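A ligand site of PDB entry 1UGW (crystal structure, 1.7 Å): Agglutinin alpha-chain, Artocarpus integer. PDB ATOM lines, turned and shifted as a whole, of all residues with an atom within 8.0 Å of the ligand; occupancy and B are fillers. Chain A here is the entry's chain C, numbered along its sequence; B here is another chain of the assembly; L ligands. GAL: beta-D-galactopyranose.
An oxygen (O6) of the ligand is in hydrogen-bond range of the backbone NH (N) of Trp 123 (3.0 Å).
The backbone NH (N) of Gly 1 sits at hydrogen-bond distance from an oxygen (O4) of the ligand, 2.9 Å away.
O of Trp 123 lies within hydrogen-bond range of O6 of the ligand (3.2 Å).
The backbone NH of Tyr 122 is in hydrogen-bond range of an oxygen (O6) of the ligand, 3.1 Å away.
The side-chain carboxylate (OD1) of Asp 125 lies within hydrogen-bond range of an oxygen (O6) of the ligand, at 2.8 Å.
Merely in contact with the ligand: Phe 47 (3.5 Å), Tyr 78 (3.7 Å), Val 80 (3.9 Å) and Gly 121 (3.6 Å).
Eight residues have an atom within 4 Å of the ligand: Gly 1, Phe 47, Tyr 78, Val 80, Gly 121, Tyr 122, Trp 123 and Asp 125.
The nearest printed residue that does not touch the ligand is Ile 120 (4.8 Å).
The backbone NH (N) of Gly 121 sits at hydrogen-bond distance from the side-chain carboxylate (OD2) of Asp 125.
O of Tyr 122 sits at hydrogen-bond distance from OG of Ser 46 (2.6 Å).
The backbone carbonyl oxygen (O) of Asp 125 sits at hydrogen-bond distance from the backbone NH (N) of Ala 17 of chain B, 2.8 Å away.
The backbone NH (N) of Phe 47 lies within hydrogen-bond range of the backbone carbonyl oxygen (O) of Gly 121, 2.8 Å away.
The backbone carbonyl oxygen (O) of Ser 119 lies within hydrogen-bond range of the backbone NH (N) of Asp 125 (2.8 Å).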
ATOM      1  N   GLY A   1     -15.538 -20.513 -14.055  1.00  0.00           N
ATOM      2  CA  GLY A   1     -15.425 -21.994 -14.115  1.00  0.00           C
ATOM      3  C   GLY A   1     -16.132 -22.597 -15.313  1.00  0.00           C
ATOM      4  O   GLY A   1     -16.710 -21.871 -16.135  1.00  0.00           O
ATOM      5  N   LYS A   2     -16.084 -23.917 -15.421  1.00  0.00           N
ATOM      6  CA  LYS A   2     -16.728 -24.627 -16.526  1.00  0.00           C
ATOM      7  C   LYS A   2     -18.142 -25.005 -16.117  1.00  0.00           C
ATOM      8  O   LYS A   2     -18.346 -25.790 -15.191  1.00  0.00           O
ATOM      9  CB  LYS A   2     -15.921 -25.877 -16.883  1.00  0.00           C
ATOM     10  CG  LYS A   2     -16.333 -26.550 -18.173  1.00  0.00           C
ATOM     11  CD  LYS A   2     -15.464 -27.765 -18.455  1.00  0.00           C
ATOM     12  CE  LYS A   2     -15.649 -28.265 -19.881  1.00  0.00           C
ATOM     13  NZ  LYS A   2     -17.075 -28.558 -20.198  1.00  0.00           N
ATOM     14  N   ALA A  24     -13.170 -25.135  -0.190  1.00  0.00           N
ATOM     15  CA  ALA A  24     -14.570 -25.336  -0.540  1.00  0.00           C
ATOM     16  C   ALA A  24     -14.809 -26.673  -1.217  1.00  0.00           C
ATOM     17  O   ALA A  24     -13.960 -27.569  -1.201  1.00  0.00           O
ATOM     18  CB  ALA A  24     -15.027 -24.200  -1.444  1.00  0.00           C
ATOM     19  N   ILE A  25     -15.990 -26.800  -1.828  1.00  0.00           N
ATOM     20  CA  ILE A  25     -16.383 -28.012  -2.536  1.00  0.00           C
ATOM     21  C   ILE A  25     -15.644 -28.054  -3.871  1.00  0.00           C
ATOM     22  O   ILE A  25     -15.512 -27.021  -4.535  1.00  0.00           O
ATOM     23  CB  ILE A  25     -17.907 -28.028  -2.822  1.00  0.00           C
ATOM     24  CG1 ILE A  25     -18.691 -27.954  -1.501  1.00  0.00           C
ATOM     25  CG2 ILE A  25     -18.279 -29.282  -3.613  1.00  0.00           C
ATOM     26  CD1 ILE A  25     -18.507 -29.151  -0.596  1.00  0.00           C
ATOM     27  N   SER A  46     -12.870 -30.368 -10.516  1.00  0.00           N
ATOM     28  CA  SER A  46     -12.208 -29.102 -10.240  1.00  0.00           C
ATOM     29  C   SER A  46     -10.965 -29.024 -11.128  1.00  0.00           C
ATOM     30  O   SER A  46     -10.457 -30.058 -11.567  1.00  0.00           O
ATOM     31  CB  SER A  46     -11.763 -29.049  -8.781  1.00  0.00           C
ATOM     32  OG  SER A  46     -10.739 -28.090  -8.599  1.00  0.00           O
ATOM     33  N   PHE A  47     -10.489 -27.804 -11.377  1.00  0.00           N
ATOM     34  CA  PHE A  47      -9.297 -27.607 -12.190  1.00  0.00           C
ATOM     35  C   PHE A  47      -8.053 -28.042 -11.426  1.00  0.00           C
ATOM     36  O   PHE A  47      -6.978 -28.177 -12.019  1.00  0.00           O
ATOM     37  CB  PHE A  47      -9.127 -26.136 -12.574  1.00  0.00           C
ATOM     38  CG  PHE A  47     -10.215 -25.589 -13.457  1.00  0.00           C
ATOM     39  CD1 PHE A  47     -11.042 -26.429 -14.194  1.00  0.00           C
ATOM     40  CD2 PHE A  47     -10.377 -24.213 -13.586  1.00  0.00           C
ATOM     41  CE1 PHE A  47     -12.014 -25.908 -15.053  1.00  0.00           C
ATOM     42  CE2 PHE A  47     -11.340 -23.676 -14.432  1.00  0.00           C
ATOM     43  CZ  PHE A  47     -12.157 -24.526 -15.173  1.00  0.00           C
ATOM     44  N   ILE A  48      -8.180 -28.241 -10.115  1.00  0.00           N
ATOM     45  CA  ILE A  48      -7.044 -28.658  -9.306  1.00  0.00           C
ATOM     46  C   ILE A  48      -7.339 -29.931  -8.510  1.00  0.00           C
ATOM     47  O   ILE A  48      -8.423 -30.494  -8.623  1.00  0.00           O
ATOM     48  CB  ILE A  48      -6.602 -27.547  -8.310  1.00  0.00           C
ATOM     49  CG1 ILE A  48      -7.763 -27.176  -7.381  1.00  0.00           C
ATOM     50  CG2 ILE A  48      -6.140 -26.318  -9.093  1.00  0.00           C
ATOM     51  CD1 ILE A  48      -7.379 -26.170  -6.297  1.00  0.00           C
ATOM     52  N   VAL A  75     -13.405 -17.228  -1.426  1.00  0.00           N
ATOM     53  CA  VAL A  75     -12.205 -18.048  -1.321  1.00  0.00           C
ATOM     54  C   VAL A  75     -11.266 -17.543  -2.413  1.00  0.00           C
ATOM     55  O   VAL A  75     -11.565 -17.664  -3.599  1.00  0.00           O
ATOM     56  CB  VAL A  75     -12.501 -19.548  -1.559  1.00  0.00           C
ATOM     57  CG1 VAL A  75     -11.211 -20.353  -1.495  1.00  0.00           C
ATOM     58  CG2 VAL A  75     -13.483 -20.057  -0.517  1.00  0.00           C
ATOM     59  N   SER A  76     -10.141 -16.962  -2.011  1.00  0.00           N
ATOM     60  CA  SER A  76      -9.165 -16.433  -2.955  1.00  0.00           C
ATOM     61  C   SER A  76      -9.780 -15.415  -3.902  1.00  0.00           C
ATOM     62  O   SER A  76      -9.417 -15.360  -5.076  1.00  0.00           O
ATOM     63  CB  SER A  76      -8.521 -17.569  -3.753  1.00  0.00           C
ATOM     64  OG  SER A  76      -7.743 -18.408  -2.918  1.00  0.00           O
ATOM     65  N   GLY A  77     -10.715 -14.626  -3.400  1.00  0.00           N
ATOM     66  CA  GLY A  77     -11.354 -13.606  -4.219  1.00  0.00           C
ATOM     67  C   GLY A  77     -12.558 -14.075  -5.019  1.00  0.00           C
ATOM     68  O   GLY A  77     -13.167 -13.282  -5.744  1.00  0.00           O
ATOM     69  N   TYR A  78     -12.903 -15.351  -4.905  1.00  0.00           N
ATOM     70  CA  TYR A  78     -14.038 -15.902  -5.631  1.00  0.00           C
ATOM     71  C   TYR A  78     -15.165 -16.331  -4.696  1.00  0.00           C
ATOM     72  O   TYR A  78     -14.919 -16.909  -3.645  1.00  0.00           O
ATOM     73  CB  TYR A  78     -13.612 -17.114  -6.460  1.00  0.00           C
ATOM     74  CG  TYR A  78     -12.572 -16.827  -7.508  1.00  0.00           C
ATOM     75  CD1 TYR A  78     -12.875 -16.068  -8.640  1.00  0.00           C
ATOM     76  CD2 TYR A  78     -11.268 -17.306  -7.378  1.00  0.00           C
ATOM     77  CE1 TYR A  78     -11.923 -15.787  -9.605  1.00  0.00           C
ATOM     78  CE2 TYR A  78     -10.296 -17.036  -8.344  1.00  0.00           C
ATOM     79  CZ  TYR A  78     -10.635 -16.281  -9.451  1.00  0.00           C
ATOM     80  OH  TYR A  78      -9.674 -16.016 -10.411  1.00  0.00           O
ATOM     81  N   VAL A  79     -16.401 -16.031  -5.083  1.00  0.00           N
ATOM     82  CA  VAL A  79     -17.552 -16.433  -4.283  1.00  0.00           C
ATOM     83  C   VAL A  79     -17.848 -17.857  -4.751  1.00  0.00           C
ATOM     84  O   VAL A  79     -18.100 -18.092  -5.926  1.00  0.00           O
ATOM     85  CB  VAL A  79     -18.776 -15.540  -4.541  1.00  0.00           C
ATOM     86  CG1 VAL A  79     -19.978 -16.070  -3.763  1.00  0.00           C
ATOM     87  CG2 VAL A  79     -18.462 -14.112  -4.115  1.00  0.00           C
ATOM     88  N   VAL A  80     -17.795 -18.811  -3.820  1.00  0.00           N
ATOM     89  CA  VAL A  80     -18.033 -20.207  -4.145  1.00  0.00           C
ATOM     90  C   VAL A  80     -18.876 -20.898  -3.077  1.00  0.00           C
ATOM     91  O   VAL A  80     -19.184 -20.318  -2.040  1.00  0.00           O
ATOM     92  CB  VAL A  80     -16.695 -20.985  -4.271  1.00  0.00           C
ATOM     93  CG1 VAL A  80     -15.853 -20.409  -5.402  1.00  0.00           C
ATOM     94  CG2 VAL A  80     -15.924 -20.891  -2.946  1.00  0.00           C
ATOM     95  N   VAL A  81     -19.259 -22.147  -3.356  1.00  0.00           N
ATOM     96  CA  VAL A  81     -20.029 -22.939  -2.407  1.00  0.00           C
ATOM     97  C   VAL A  81     -18.985 -23.629  -1.542  1.00  0.00           C
ATOM     98  O   VAL A  81     -18.263 -24.508  -1.998  1.00  0.00           O
ATOM     99  CB  VAL A  81     -20.910 -23.965  -3.132  1.00  0.00           C
ATOM    100  CG1 VAL A  81     -21.659 -24.820  -2.120  1.00  0.00           C
ATOM    101  CG2 VAL A  81     -21.903 -23.247  -4.039  1.00  0.00           C
ATOM    102  N   SER A 119     -21.560 -24.673 -12.076  1.00  0.00           N
ATOM    103  CA  SER A 119     -20.265 -24.372 -12.661  1.00  0.00           C
ATOM    104  C   SER A 119     -19.155 -24.709 -11.662  1.00  0.00           C
ATOM    105  O   SER A 119     -19.319 -24.503 -10.465  1.00  0.00           O
ATOM    106  CB  SER A 119     -20.189 -22.882 -13.021  1.00  0.00           C
ATOM    107  OG  SER A 119     -18.875 -22.517 -13.391  1.00  0.00           O
ATOM    108  N   ILE A 120     -18.047 -25.224 -12.162  1.00  0.00           N
ATOM    109  CA  ILE A 120     -16.909 -25.576 -11.324  1.00  0.00           C
ATOM    110  C   ILE A 120     -15.602 -25.140 -11.953  1.00  0.00           C
ATOM    111  O   ILE A 120     -15.314 -25.465 -13.110  1.00  0.00           O
ATOM    112  CB  ILE A 120     -16.827 -27.104 -11.070  1.00  0.00           C
ATOM    113  CG1 ILE A 120     -18.092 -27.614 -10.380  1.00  0.00           C
ATOM    114  CG2 ILE A 120     -15.609 -27.434 -10.209  1.00  0.00           C
ATOM    115  CD1 ILE A 120     -18.096 -29.119 -10.146  1.00  0.00           C
ATOM    116  N   GLY A 121     -14.806 -24.380 -11.203  1.00  0.00           N
ATOM    117  CA  GLY A 121     -13.506 -23.948 -11.678  1.00  0.00           C
ATOM    118  C   GLY A 121     -12.563 -24.621 -10.694  1.00  0.00           C
ATOM    119  O   GLY A 121     -12.430 -25.847 -10.707  1.00  0.00           O
ATOM    120  N   TYR A 122     -11.916 -23.841  -9.846  1.00  0.00           N
ATOM    121  CA  TYR A 122     -11.061 -24.428  -8.829  1.00  0.00           C
ATOM    122  C   TYR A 122     -12.039 -25.071  -7.837  1.00  0.00           C
ATOM    123  O   TYR A 122     -11.760 -26.114  -7.245  1.00  0.00           O
ATOM    124  CB  TYR A 122     -10.257 -23.346  -8.100  1.00  0.00           C
ATOM    125  CG  TYR A 122      -9.065 -22.814  -8.880  1.00  0.00           C
ATOM    126  CD1 TYR A 122      -8.320 -21.744  -8.392  1.00  0.00           C
ATOM    127  CD2 TYR A 122      -8.666 -23.398 -10.078  1.00  0.00           C
ATOM    128  CE1 TYR A 122      -7.195 -21.277  -9.072  1.00  0.00           C
ATOM    129  CE2 TYR A 122      -7.550 -22.947 -10.770  1.00  0.00           C
ATOM    130  CZ  TYR A 122      -6.819 -21.886 -10.268  1.00  0.00           C
ATOM    131  OH  TYR A 122      -5.698 -21.446 -10.942  1.00  0.00           O
ATOM    132  N   TRP A 123     -13.193 -24.422  -7.675  1.00  0.00           N
ATOM    133  CA  TRP A 123     -14.220 -24.890  -6.752  1.00  0.00           C
ATOM    134  C   TRP A 123     -15.606 -24.763  -7.373  1.00  0.00           C
ATOM    135  O   TRP A 123     -15.767 -24.211  -8.456  1.00  0.00           O
ATOM    136  CB  TRP A 123     -14.153 -24.084  -5.451  1.00  0.00           C
ATOM    137  CG  TRP A 123     -12.788 -24.103  -4.815  1.00  0.00           C
ATOM    138  CD1 TRP A 123     -12.190 -25.164  -4.191  1.00  0.00           C
ATOM    139  CD2 TRP A 123     -11.819 -23.056  -4.845  1.00  0.00           C
ATOM    140  NE1 TRP A 123     -10.902 -24.833  -3.823  1.00  0.00           N
ATOM    141  CE2 TRP A 123     -10.647 -23.545  -4.219  1.00  0.00           C
ATOM    142  CE3 TRP A 123     -11.820 -21.742  -5.337  1.00  0.00           C
ATOM    143  CZ2 TRP A 123      -9.485 -22.766  -4.069  1.00  0.00           C
ATOM    144  CZ3 TRP A 123     -10.658 -20.972  -5.193  1.00  0.00           C
ATOM    145  CH2 TRP A 123      -9.519 -21.485  -4.567  1.00  0.00           C
ATOM    146  N   LEU A 124     -16.608 -25.296  -6.680  1.00  0.00           N
ATOM    147  CA  LEU A 124     -17.999 -25.223  -7.142  1.00  0.00           C
ATOM    148  C   LEU A 124     -18.419 -23.752  -7.032  1.00  0.00           C
ATOM    149  O   LEU A 124     -18.584 -23.220  -5.918  1.00  0.00           O
ATOM    150  CB  LEU A 124     -18.888 -26.108  -6.271  1.00  0.00           C
ATOM    151  CG  LEU A 124     -20.395 -26.115  -6.535  1.00  0.00           C
ATOM    152  CD1 LEU A 124     -20.689 -26.593  -7.961  1.00  0.00           C
ATOM    153  CD2 LEU A 124     -21.081 -27.045  -5.519  1.00  0.00           C
ATOM    154  N   ASP A 125     -18.580 -23.095  -8.170  1.00  0.00           N
ATOM    155  CA  ASP A 125     -18.949 -21.676  -8.201  1.00  0.00           C
ATOM    156  C   ASP A 125     -20.396 -21.422  -7.796  1.00  0.00           C
ATOM    157  O   ASP A 125     -20.671 -20.507  -7.022  1.00  0.00           O
ATOM    158  CB  ASP A 125     -18.714 -21.109  -9.601  1.00  0.00           C
ATOM    159  CG  ASP A 125     -17.279 -21.270 -10.058  1.00  0.00           C
ATOM    160  OD1 ASP A 125     -16.366 -20.858  -9.320  1.00  0.00           O
ATOM    161  OD2 ASP A 125     -17.065 -21.807 -11.164  1.00  0.00           O
ATOM    162  N   TYR A 126     -21.308 -22.220  -8.321  1.00  0.00           N
ATOM    163  CA  TYR A 126     -22.718 -22.081  -8.016  1.00  0.00           C
ATOM    164  C   TYR A 126     -23.435 -23.313  -8.528  1.00  0.00           C
ATOM    165  O   TYR A 126     -22.870 -24.088  -9.296  1.00  0.00           O
ATOM    166  CB  TYR A 126     -23.288 -20.819  -8.674  1.00  0.00           C
ATOM    167  CG  TYR A 126     -23.160 -20.772 -10.191  1.00  0.00           C
ATOM    168  CD1 TYR A 126     -24.004 -21.532 -11.014  1.00  0.00           C
ATOM    169  CD2 TYR A 126     -22.186 -19.975 -10.794  1.00  0.00           C
ATOM    170  CE1 TYR A 126     -23.870 -21.496 -12.404  1.00  0.00           C
ATOM    171  CE2 TYR A 126     -22.052 -19.930 -12.177  1.00  0.00           C
ATOM    172  CZ  TYR A 126     -22.890 -20.694 -12.977  1.00  0.00           C
ATOM    173  OH  TYR A 126     -22.749 -20.647 -14.346  1.00  0.00           O
ATOM    174  N   ALA B  17     -21.819 -17.973  -6.594  1.00  0.00           N
ATOM    175  CA  ALA B  17     -21.427 -16.797  -7.368  1.00  0.00           C
ATOM    176  C   ALA B  17     -22.574 -16.322  -8.251  1.00  0.00           C
ATOM    177  O   ALA B  17     -23.449 -17.095  -8.629  1.00  0.00           O
ATOM    178  CB  ALA B  17     -20.202 -17.127  -8.231  1.00  0.00           C
HETATM  179  C1  GAL L   1     -10.968 -20.315 -11.241  1.00  0.00           C
HETATM  180  C2  GAL L   1     -11.749 -19.894 -12.481  1.00  0.00           C
HETATM  181  C3  GAL L   1     -12.809 -18.863 -12.098  1.00  0.00           C
HETATM  182  C4  GAL L   1     -13.684 -19.369 -10.967  1.00  0.00           C
HETATM  183  C5  GAL L   1     -12.796 -19.752  -9.786  1.00  0.00           C
HETATM  184  C6  GAL L   1     -13.573 -20.312  -8.604  1.00  0.00           C
HETATM  185  O1  GAL L   1     -10.175 -21.394 -11.589  1.00  0.00           O
HETATM  186  O2  GAL L   1     -10.851 -19.297 -13.402  1.00  0.00           O
HETATM  187  O3  GAL L   1     -13.616 -18.533 -13.195  1.00  0.00           O
HETATM  188  O4  GAL L   1     -14.412 -20.508 -11.421  1.00  0.00           O
HETATM  189  O5  GAL L   1     -11.863 -20.760 -10.186  1.00  0.00           O
HETATM  190  O6  GAL L   1     -13.804 -21.711  -8.686  1.00  0.00           O
